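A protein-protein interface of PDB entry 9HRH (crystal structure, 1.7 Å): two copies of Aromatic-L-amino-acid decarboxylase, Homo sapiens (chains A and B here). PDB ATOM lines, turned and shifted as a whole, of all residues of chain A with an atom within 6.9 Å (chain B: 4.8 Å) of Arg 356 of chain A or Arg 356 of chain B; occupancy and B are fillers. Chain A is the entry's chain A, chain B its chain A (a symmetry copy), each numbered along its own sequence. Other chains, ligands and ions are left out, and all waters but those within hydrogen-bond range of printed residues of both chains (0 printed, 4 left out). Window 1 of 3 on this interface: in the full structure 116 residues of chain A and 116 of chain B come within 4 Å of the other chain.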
ATOM      1  N   ASP A  92      19.382 -29.638  20.334  1.00  0.00           N
ATOM      2  CA  ASP A  92      19.332 -28.249  20.768  1.00  0.00           C
ATOM      3  C   ASP A  92      20.614 -27.510  20.402  1.00  0.00           C
ATOM      4  O   ASP A  92      20.576 -26.306  20.120  1.00  0.00           O
ATOM      5  CB  ASP A  92      19.085 -28.182  22.273  1.00  0.00           C
ATOM      6  CG  ASP A  92      17.948 -27.242  22.634  1.00  0.00           C
ATOM      7  OD1 ASP A  92      17.528 -27.248  23.810  1.00  0.00           O
ATOM      8  OD2 ASP A  92      17.446 -26.535  21.735  1.00  0.00           O
ATOM      9  N   CYS A  95      20.015 -26.743  16.844  1.00  0.00           N
ATOM     10  CA  CYS A  95      18.982 -25.716  16.748  1.00  0.00           C
ATOM     11  C   CYS A  95      19.566 -24.321  16.933  1.00  0.00           C
ATOM     12  O   CYS A  95      19.221 -23.392  16.192  1.00  0.00           O
ATOM     13  CB  CYS A  95      17.890 -25.984  17.784  1.00  0.00           C
ATOM     14  SG  CYS A  95      16.559 -24.767  17.815  1.00  0.00           S
ATOM     15  N   GLY A  96      20.448 -24.151  17.922  1.00  0.00           N
ATOM     16  CA  GLY A  96      21.091 -22.864  18.116  1.00  0.00           C
ATOM     17  C   GLY A  96      22.078 -22.530  17.018  1.00  0.00           C
ATOM     18  O   GLY A  96      22.354 -21.354  16.765  1.00  0.00           O
ATOM     19  N   CYS A 100      17.519 -20.287  13.133  1.00  0.00           N
ATOM     20  CA  CYS A 100      16.449 -19.672  12.366  1.00  0.00           C
ATOM     21  C   CYS A 100      15.318 -19.226  13.286  1.00  0.00           C
ATOM     22  O   CYS A 100      15.103 -19.784  14.365  1.00  0.00           O
ATOM     23  CB  CYS A 100      15.901 -20.638  11.311  1.00  0.00           C
ATOM     24  SG  CYS A 100      15.323 -22.236  11.952  1.00  0.00           S
ATOM     25  N   ILE A 101      14.590 -18.206  12.838  1.00  0.00           N
ATOM     26  CA  ILE A 101      13.381 -17.757  13.515  1.00  0.00           C
ATOM     27  C   ILE A 101      12.215 -18.052  12.585  1.00  0.00           C
ATOM     28  O   ILE A 101      11.889 -17.247  11.707  1.00  0.00           O
ATOM     29  CB  ILE A 101      13.453 -16.262  13.875  1.00  0.00           C
ATOM     30  CG1 ILE A 101      14.694 -15.982  14.721  1.00  0.00           C
ATOM     31  CG2 ILE A 101      12.205 -15.838  14.629  1.00  0.00           C
ATOM     32  CD1 ILE A 101      14.716 -16.739  16.034  1.00  0.00           C
ATOM     33  N   GLY A 102      11.590 -19.212  12.758  1.00  0.00           N
ATOM     34  CA  GLY A 102      10.590 -19.666  11.814  1.00  0.00           C
ATOM     35  C   GLY A 102       9.213 -19.056  11.985  1.00  0.00           C
ATOM     36  O   GLY A 102       8.230 -19.783  12.149  1.00  0.00           O
ATOM     37  N   CYS A 111      12.233 -25.706   9.162  1.00  0.00           N
ATOM     38  CA  CYS A 111      11.774 -25.512  10.534  1.00  0.00           C
ATOM     39  C   CYS A 111      10.278 -25.776  10.656  1.00  0.00           C
ATOM     40  O   CYS A 111       9.818 -26.347  11.651  1.00  0.00           O
ATOM     41  CB  CYS A 111      12.116 -24.097  11.004  1.00  0.00           C
ATOM     42  SG  CYS A 111      11.577 -23.693  12.692  1.00  0.00           S
ATOM     43  N   GLU A 115       8.359 -29.882  11.716  1.00  0.00           N
ATOM     44  CA  GLU A 115       7.404 -29.827  12.818  1.00  0.00           C
ATOM     45  C   GLU A 115       6.095 -30.511  12.449  1.00  0.00           C
ATOM     46  O   GLU A 115       5.540 -31.277  13.247  1.00  0.00           O
ATOM     47  CB  GLU A 115       7.154 -28.374  13.223  1.00  0.00           C
ATOM     48  CG  GLU A 115       6.276 -28.226  14.451  1.00  0.00           C
ATOM     49  CD  GLU A 115       6.395 -26.859  15.092  1.00  0.00           C
ATOM     50  OE1 GLU A 115       7.530 -26.341  15.186  1.00  0.00           O
ATOM     51  OE2 GLU A 115       5.356 -26.311  15.516  1.00  0.00           O
ATOM     52  N   ILE A 144       3.802 -27.289  17.689  1.00  0.00           N
ATOM     53  CA  ILE A 144       4.523 -27.203  18.953  1.00  0.00           C
ATOM     54  C   ILE A 144       4.200 -25.873  19.619  1.00  0.00           C
ATOM     55  O   ILE A 144       4.328 -24.808  19.004  1.00  0.00           O
ATOM     56  CB  ILE A 144       6.037 -27.349  18.738  1.00  0.00           C
ATOM     57  CG1 ILE A 144       6.372 -28.697  18.103  1.00  0.00           C
ATOM     58  CG2 ILE A 144       6.772 -27.180  20.059  1.00  0.00           C
ATOM     59  CD1 ILE A 144       7.809 -28.791  17.648  1.00  0.00           C
ATOM     60  N   ASN A 308      13.546 -32.203  25.824  1.00  0.00           N
ATOM     61  CA  ASN A 308      13.860 -31.099  26.730  1.00  0.00           C
ATOM     62  C   ASN A 308      12.979 -29.880  26.473  1.00  0.00           C
ATOM     63  O   ASN A 308      12.686 -29.534  25.325  1.00  0.00           O
ATOM     64  CB  ASN A 308      15.333 -30.703  26.591  1.00  0.00           C
ATOM     65  CG  ASN A 308      16.284 -31.847  26.894  1.00  0.00           C
ATOM     66  OD1 ASN A 308      15.865 -32.984  27.108  1.00  0.00           O
ATOM     67  ND2 ASN A 308      17.579 -31.550  26.898  1.00  0.00           N
ATOM     68  N   PHE A 309      12.555 -29.240  27.565  1.00  0.00           N
ATOM     69  CA  PHE A 309      11.788 -27.998  27.504  1.00  0.00           C
ATOM     70  C   PHE A 309      12.534 -26.967  26.664  1.00  0.00           C
ATOM     71  O   PHE A 309      13.749 -26.803  26.810  1.00  0.00           O
ATOM     72  CB  PHE A 309      11.566 -27.495  28.938  1.00  0.00           C
ATOM     73  CG  PHE A 309      10.680 -26.283  29.057  1.00  0.00           C
ATOM     74  CD1 PHE A 309      11.188 -25.011  28.878  1.00  0.00           C
ATOM     75  CD2 PHE A 309       9.346 -26.418  29.405  1.00  0.00           C
ATOM     76  CE1 PHE A 309      10.383 -23.896  29.008  1.00  0.00           C
ATOM     77  CE2 PHE A 309       8.531 -25.307  29.537  1.00  0.00           C
ATOM     78  CZ  PHE A 309       9.053 -24.043  29.338  1.00  0.00           C
ATOM     79  N   ASP A 310      11.818 -26.269  25.780  1.00  0.00           N
ATOM     80  CA  ASP A 310      10.361 -26.323  25.655  1.00  0.00           C
ATOM     81  C   ASP A 310       9.860 -27.151  24.470  1.00  0.00           C
ATOM     82  O   ASP A 310      10.402 -27.073  23.368  1.00  0.00           O
ATOM     83  CB  ASP A 310       9.806 -24.900  25.544  1.00  0.00           C
ATOM     84  CG  ASP A 310      10.513 -24.079  24.476  1.00  0.00           C
ATOM     85  OD1 ASP A 310      11.728 -24.291  24.270  1.00  0.00           O
ATOM     86  OD2 ASP A 310       9.859 -23.225  23.841  1.00  0.00           O
ATOM     87  N   CYS A 311       8.807 -27.938  24.715  1.00  0.00           N
ATOM     88  CA  CYS A 311       8.153 -28.724  23.667  1.00  0.00           C
ATOM     89  C   CYS A 311       6.790 -29.168  24.197  1.00  0.00           C
ATOM     90  O   CYS A 311       6.711 -30.131  24.963  1.00  0.00           O
ATOM     91  CB  CYS A 311       8.993 -29.919  23.249  1.00  0.00           C
ATOM     92  SG  CYS A 311       8.250 -30.874  21.896  1.00  0.00           S
ATOM     93  N   GLY A 354       7.594 -15.407  16.699  1.00  0.00           N
ATOM     94  CA  GLY A 354       8.844 -16.100  16.489  1.00  0.00           C
ATOM     95  C   GLY A 354       8.900 -17.435  17.210  1.00  0.00           C
ATOM     96  O   GLY A 354       8.187 -17.672  18.184  1.00  0.00           O
ATOM     97  N   ARG A 355       9.760 -18.322  16.707  1.00  0.00           N
ATOM     98  CA  ARG A 355       9.891 -19.656  17.278  1.00  0.00           C
ATOM     99  C   ARG A 355      11.217 -20.269  16.850  1.00  0.00           C
ATOM    100  O   ARG A 355      11.809 -19.876  15.841  1.00  0.00           O
ATOM    101  CB  ARG A 355       8.726 -20.560  16.858  1.00  0.00           C
ATOM    102  CG  ARG A 355       8.503 -20.618  15.354  1.00  0.00           C
ATOM    103  CD  ARG A 355       7.019 -20.668  15.031  1.00  0.00           C
ATOM    104  NE  ARG A 355       6.323 -21.648  15.854  1.00  0.00           N
ATOM    105  CZ  ARG A 355       6.350 -22.957  15.648  1.00  0.00           C
ATOM    106  NH1 ARG A 355       7.017 -23.484  14.633  1.00  0.00           N
ATOM    107  NH2 ARG A 355       5.695 -23.759  16.484  1.00  0.00           N
ATOM    108  N   ARG A 356      11.670 -21.244  17.637  1.00  0.00           N
ATOM    109  CA  ARG A 356      12.890 -21.992  17.369  1.00  0.00           C
ATOM    110  C   ARG A 356      12.596 -23.252  16.562  1.00  0.00           C
ATOM    111  O   ARG A 356      11.445 -23.647  16.365  1.00  0.00           O
ATOM    112  CB  ARG A 356      13.591 -22.388  18.669  1.00  0.00           C
ATOM    113  CG  ARG A 356      14.012 -21.242  19.546  1.00  0.00           C
ATOM    114  CD  ARG A 356      15.009 -21.695  20.597  1.00  0.00           C
ATOM    115  NE  ARG A 356      14.385 -22.472  21.663  1.00  0.00           N
ATOM    116  CZ  ARG A 356      14.969 -23.487  22.284  1.00  0.00           C
ATOM    117  NH1 ARG A 356      16.191 -23.881  21.964  1.00  0.00           N
ATOM    118  NH2 ARG A 356      14.312 -24.123  23.249  1.00  0.00           N
ATOM    119  N   PHE A 357      13.674 -23.901  16.122  1.00  0.00           N
ATOM    120  CA  PHE A 357      13.609 -25.169  15.395  1.00  0.00           C
ATOM    121  C   PHE A 357      13.449 -26.326  16.387  1.00  0.00           C
ATOM    122  O   PHE A 357      14.239 -27.268  16.435  1.00  0.00           O
ATOM    123  CB  PHE A 357      14.861 -25.327  14.540  1.00  0.00           C
ATOM    124  CG  PHE A 357      14.709 -26.269  13.368  1.00  0.00           C
ATOM    125  CD1 PHE A 357      13.661 -27.174  13.296  1.00  0.00           C
ATOM    126  CD2 PHE A 357      15.635 -26.244  12.335  1.00  0.00           C
ATOM    127  CE1 PHE A 357      13.541 -28.035  12.213  1.00  0.00           C
ATOM    128  CE2 PHE A 357      15.518 -27.099  11.252  1.00  0.00           C
ATOM    129  CZ  PHE A 357      14.470 -27.994  11.191  1.00  0.00           C
ATOM    130  N   ARG A 358      12.391 -26.234  17.198  1.00  0.00           N
ATOM    131  CA  ARG A 358      12.190 -27.186  18.287  1.00  0.00           C
ATOM    132  C   ARG A 358      11.842 -28.586  17.798  1.00  0.00           C
ATOM    133  O   ARG A 358      12.013 -29.548  18.554  1.00  0.00           O
ATOM    134  CB  ARG A 358      11.101 -26.677  19.234  1.00  0.00           C
ATOM    135  CG  ARG A 358      11.468 -25.382  19.946  1.00  0.00           C
ATOM    136  CD  ARG A 358      10.303 -24.821  20.750  1.00  0.00           C
ATOM    137  NE  ARG A 358       9.194 -24.422  19.893  1.00  0.00           N
ATOM    138  CZ  ARG A 358       8.211 -23.611  20.266  1.00  0.00           C
ATOM    139  NH1 ARG A 358       8.159 -23.105  21.487  1.00  0.00           N
ATOM    140  NH2 ARG A 358       7.260 -23.297  19.391  1.00  0.00           N
ATOM    141  N   SER A 359      11.366 -28.731  16.560  1.00  0.00           N
ATOM    142  CA  SER A 359      11.041 -30.060  16.056  1.00  0.00           C
ATOM    143  C   SER A 359      12.279 -30.934  15.908  1.00  0.00           C
ATOM    144  O   SER A 359      12.150 -32.162  15.843  1.00  0.00           O
ATOM    145  CB  SER A 359      10.319 -29.961  14.713  1.00  0.00           C
ATOM    146  OG  SER A 359      11.045 -29.163  13.799  1.00  0.00           O
ATOM    147  N   LYS A 361      14.406 -31.447  18.214  1.00  0.00           N
ATOM    148  CA  LYS A 361      14.477 -32.217  19.452  1.00  0.00           C
ATOM    149  C   LYS A 361      13.581 -33.448  19.393  1.00  0.00           C
ATOM    150  O   LYS A 361      14.003 -34.543  19.782  1.00  0.00           O
ATOM    151  CB  LYS A 361      14.112 -31.347  20.655  1.00  0.00           C
ATOM    152  CG  LYS A 361      15.167 -30.321  21.037  1.00  0.00           C
ATOM    153  CD  LYS A 361      14.737 -29.547  22.274  1.00  0.00           C
ATOM    154  CE  LYS A 361      13.509 -28.689  22.007  1.00  0.00           C
ATOM    155  NZ  LYS A 361      13.181 -27.842  23.192  1.00  0.00           N
ATOM    156  N   ASP B  92      23.650 -22.407  26.757  1.00  0.00           N
ATOM    157  CA  ASP B  92      22.446 -23.164  26.447  1.00  0.00           C
ATOM    158  C   ASP B  92      22.661 -24.657  26.667  1.00  0.00           C
ATOM    159  O   ASP B  92      21.723 -25.369  27.044  1.00  0.00           O
ATOM    160  CB  ASP B  92      22.016 -22.889  25.007  1.00  0.00           C
ATOM    161  CG  ASP B  92      20.546 -22.518  24.901  1.00  0.00           C
ATOM    162  OD1 ASP B  92      20.125 -22.089  23.807  1.00  0.00           O
ATOM    163  OD2 ASP B  92      19.829 -22.612  25.920  1.00  0.00           O
ATOM    164  N   CYS B  95      22.251 -24.915  30.322  1.00  0.00           N
ATOM    165  CA  CYS B  95      20.843 -24.715  30.657  1.00  0.00           C
ATOM    166  C   CYS B  95      20.044 -26.001  30.492  1.00  0.00           C
ATOM    167  O   CYS B  95      19.216 -26.339  31.348  1.00  0.00           O
ATOM    168  CB  CYS B  95      20.260 -23.603  29.785  1.00  0.00           C
ATOM    169  SG  CYS B  95      18.509 -23.268  30.054  1.00  0.00           S
ATOM    170  N   CYS B 100      16.222 -27.079  34.867  1.00  0.00           N
ATOM    171  CA  CYS B 100      15.224 -26.655  35.835  1.00  0.00           C
ATOM    172  C   CYS B 100      14.068 -25.948  35.138  1.00  0.00           C
ATOM    173  O   CYS B 100      14.219 -25.359  34.066  1.00  0.00           O
ATOM    174  CB  CYS B 100      15.839 -25.722  36.883  1.00  0.00           C
ATOM    175  SG  CYS B 100      16.676 -24.255  36.218  1.00  0.00           S
ATOM    176  N   CYS B 111      18.070 -19.931  39.172  1.00  0.00           N
ATOM    177  CA  CYS B 111      17.435 -19.574  37.907  1.00  0.00           C
ATOM    178  C   CYS B 111      16.754 -18.214  37.999  1.00  0.00           C
ATOM    179  O   CYS B 111      16.786 -17.427  37.045  1.00  0.00           O
ATOM    180  CB  CYS B 111      16.434 -20.657  37.502  1.00  0.00           C
ATOM    181  SG  CYS B 111      15.538 -20.338  35.954  1.00  0.00           S
ATOM    182  N   PHE B 309      18.230 -16.639  20.724  1.00  0.00           N
ATOM    183  CA  PHE B 309      16.802 -16.776  20.998  1.00  0.00           C
ATOM    184  C   PHE B 309      16.545 -18.054  21.790  1.00  0.00           C
ATOM    185  O   PHE B 309      17.100 -19.109  21.471  1.00  0.00           O
ATOM    186  CB  PHE B 309      16.050 -16.790  19.658  1.00  0.00           C
ATOM    187  CG  PHE B 309      14.548 -16.800  19.773  1.00  0.00           C
ATOM    188  CD1 PHE B 309      13.858 -17.980  19.970  1.00  0.00           C
ATOM    189  CD2 PHE B 309      13.824 -15.627  19.626  1.00  0.00           C
ATOM    190  CE1 PHE B 309      12.480 -17.994  20.053  1.00  0.00           C
ATOM    191  CE2 PHE B 309      12.441 -15.633  19.709  1.00  0.00           C
ATOM    192  CZ  PHE B 309      11.770 -16.821  19.923  1.00  0.00           C
ATOM    193  N   ASP B 310      15.706 -17.969  22.826  1.00  0.00           N
ATOM    194  CA  ASP B 310      14.918 -16.786  23.170  1.00  0.00           C
ATOM    195  C   ASP B 310      15.470 -15.983  24.350  1.00  0.00           C
ATOM    196  O   ASP B 310      15.894 -16.548  25.358  1.00  0.00           O
ATOM    197  CB  ASP B 310      13.478 -17.204  23.476  1.00  0.00           C
ATOM    198  CG  ASP B 310      13.401 -18.342  24.482  1.00  0.00           C
ATOM    199  OD1 ASP B 310      14.311 -19.199  24.480  1.00  0.00           O
ATOM    200  OD2 ASP B 310      12.438 -18.382  25.275  1.00  0.00           O
ATOM    201  N   GLY B 354       5.988 -21.813  33.268  1.00  0.00           N
ATOM    202  CA  GLY B 354       7.302 -22.411  33.228  1.00  0.00           C
ATOM    203  C   GLY B 354       8.287 -21.600  32.404  1.00  0.00           C
ATOM    204  O   GLY B 354       7.909 -20.814  31.537  1.00  0.00           O
ATOM    205  N   ARG B 355       9.573 -21.793  32.698  1.00  0.00           N
ATOM    206  CA  ARG B 355      10.625 -21.054  32.012  1.00  0.00           C
ATOM    207  C   ARG B 355      11.954 -21.778  32.181  1.00  0.00           C
ATOM    208  O   ARG B 355      12.141 -22.564  33.114  1.00  0.00           O
ATOM    209  CB  ARG B 355      10.731 -19.618  32.536  1.00  0.00           C
ATOM    210  CG  ARG B 355      10.880 -19.521  34.046  1.00  0.00           C
ATOM    211  CD  ARG B 355      10.104 -18.334  34.591  1.00  0.00           C
ATOM    212  NE  ARG B 355      10.351 -17.129  33.811  1.00  0.00           N
ATOM    213  CZ  ARG B 355      11.442 -16.383  33.908  1.00  0.00           C
ATOM    214  NH1 ARG B 355      12.409 -16.676  34.763  1.00  0.00           N
ATOM    215  NH2 ARG B 355      11.569 -15.315  33.123  1.00  0.00           N
ATOM    216  N   ARG B 356      12.875 -21.494  31.260  1.00  0.00           N
ATOM    217  CA  ARG B 356      14.224 -22.041  31.277  1.00  0.00           C
ATOM    218  C   ARG B 356      15.181 -21.114  32.019  1.00  0.00           C
ATOM    219  O   ARG B 356      14.855 -19.975  32.361  1.00  0.00           O
ATOM    220  CB  ARG B 356      14.748 -22.261  29.857  1.00  0.00           C
ATOM    221  CG  ARG B 356      13.944 -23.214  29.017  1.00  0.00           C
ATOM    222  CD  ARG B 356      14.725 -23.655  27.793  1.00  0.00           C
ATOM    223  NE  ARG B 356      14.815 -22.610  26.779  1.00  0.00           N
ATOM    224  CZ  ARG B 356      15.869 -22.420  25.998  1.00  0.00           C
ATOM    225  NH1 ARG B 356      16.946 -23.182  26.094  1.00  0.00           N
ATOM    226  NH2 ARG B 356      15.843 -21.439  25.100  1.00  0.00           N
ATOM    227  N   PHE B 357      16.396 -21.619  32.236  1.00  0.00           N
ATOM    228  CA  PHE B 357      17.480 -20.863  32.863  1.00  0.00           C
ATOM    229  C   PHE B 357      18.156 -19.966  31.820  1.00  0.00           C
ATOM    230  O   PHE B 357      19.362 -20.028  31.578  1.00  0.00           O
ATOM    231  CB  PHE B 357      18.470 -21.834  33.499  1.00  0.00           C
ATOM    232  CG  PHE B 357      19.313 -21.240  34.602  1.00  0.00           C
ATOM    233  CD1 PHE B 357      19.435 -19.868  34.767  1.00  0.00           C
ATOM    234  CD2 PHE B 357      19.994 -22.073  35.480  1.00  0.00           C
ATOM    235  CE1 PHE B 357      20.217 -19.341  35.784  1.00  0.00           C
ATOM    236  CE2 PHE B 357      20.775 -21.552  36.498  1.00  0.00           C
ATOM    237  CZ  PHE B 357      20.886 -20.186  36.650  1.00  0.00           C
ATOM    238  N   ARG B 358      17.340 -19.115  31.192  1.00  0.00           N
ATOM    239  CA  ARG B 358      17.814 -18.300  30.077  1.00  0.00           C
ATOM    240  C   ARG B 358      18.802 -17.222  30.503  1.00  0.00           C
ATOM    241  O   ARG B 358      19.552 -16.724  29.657  1.00  0.00           O
ATOM    242  CB  ARG B 358      16.626 -17.663  29.351  1.00  0.00           C
ATOM    243  CG  ARG B 358      15.698 -18.676  28.695  1.00  0.00           C
ATOM    244  CD  ARG B 358      14.446 -18.020  28.126  1.00  0.00           C
ATOM    245  NE  ARG B 358      13.612 -17.442  29.174  1.00  0.00           N
ATOM    246  CZ  ARG B 358      12.336 -17.115  29.021  1.00  0.00           C
ATOM    247  NH1 ARG B 358      11.713 -17.282  27.866  1.00  0.00           N
ATOM    248  NH2 ARG B 358      11.667 -16.612  30.054  1.00  0.00           N
ATOM    249  N   LYS B 361      22.514 -17.521  29.474  1.00  0.00           N
ATOM    250  CA  LYS B 361      22.978 -17.020  28.185  1.00  0.00           C
ATOM    251  C   LYS B 361      23.446 -15.574  28.285  1.00  0.00           C
ATOM    252  O   LYS B 361      24.505 -15.224  27.751  1.00  0.00           O
ATOM    253  CB  LYS B 361      21.886 -17.157  27.123  1.00  0.00           C
ATOM    254  CG  LYS B 361      21.625 -18.583  26.664  1.00  0.00           C
ATOM    255  CD  LYS B 361      20.566 -18.606  25.573  1.00  0.00           C
ATOM    256  CE  LYS B 361      19.206 -18.162  26.092  1.00  0.00           C
ATOM    257  NZ  LYS B 361      18.157 -18.315  25.042  1.00  0.00           N
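The guanidinium group (NH1) of Arg 356 of chain A lies within salt-bridge range of the side-chain carboxylate (OD2) of Asp 92 of chain A (2.9 Å). The side-chain sulfur (SG) of Cys 111 of chain A sits at hydrogen-bond distance from the backbone carbonyl oxygen (O) of Arg 356 of chain A. NH2 of Arg 356 of chain A is in salt-bridge range of OD1 of Asp 310 of chain A, 2.8 Å away. NH1 of Arg 356 of chain B is in salt-bridge range of OD2 of Asp 92 of chain B (2.9 Å). SG of Cys 111 of chain B is in hydrogen-bond range of O of Arg 356 of chain B (3.7 Å). The guanidinium group (NH2) of Arg 356 of chain B lies within salt-bridge range of the side-chain carboxylate (OD1) of Asp 310 of chain B (2.8 Å).
Of the 20 printed residues of chain A, 4 touch a printed residue of chain B. Hydrophobic or aromatic side chains of chain A that line the printed part of chain B: Ile 101 and Phe 309. Among the printed residues, 6 pairs touch across the chains. Among the printed residues, no Asp or Glu carboxylate lies within 4 Å of a Lys or Arg side-chain nitrogen of the other chain.
Phe 309 of chain A touches Gly 354 of chain B, and with the chains exchanged Gly 354 of chain A touches Phe 309 of chain B. Phe 309 of chain A touches Arg 356 of chain B, and with the chains exchanged Arg 356 of chain A touches Phe 309 of chain B. Arg 356 of chain A touches its own counterpart, Arg 356 of chain B. 12 positions are printed for both chains. Of the 6 pairs that touch across the chains among the printed residues, 5 have their exchanged pair printed and touching as well.
Printed residues of chain A within 4 Å of Arg 356 of chain B: Phe 309 and Arg 356. Of the printed residues of chain A, Phe 309 of chain B touches Ile 101, Gly 354 and Arg 356. Printed residues of chain B within 4 Å of Ile 101 of chain A: Phe 309 (3.7 Å). Of the printed residues of chain B, Gly 354 of chain A touches Phe 309 (3.997 Å). The nearest residue of chain B that does not touch Arg 356 of chain A is Asp 310 of chain B (4.3 Å).
Among the printed residues, pairs that only touch across the chains: Ile 101 of chain A with Phe 309 of chain B (3.7 Å), Phe 309 of chain A with Gly 354 of chain B (3.99 Å), Phe 309 of chain A with Arg 356 of chain B (3.3 Å), Gly 354 of chain A with Phe 309 of chain B (3.997 Å), Arg 356 of chain A with Phe 309 of chain B (3.3 Å) and Arg 356 of chain A with Arg 356 of chain B (3.6 Å).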
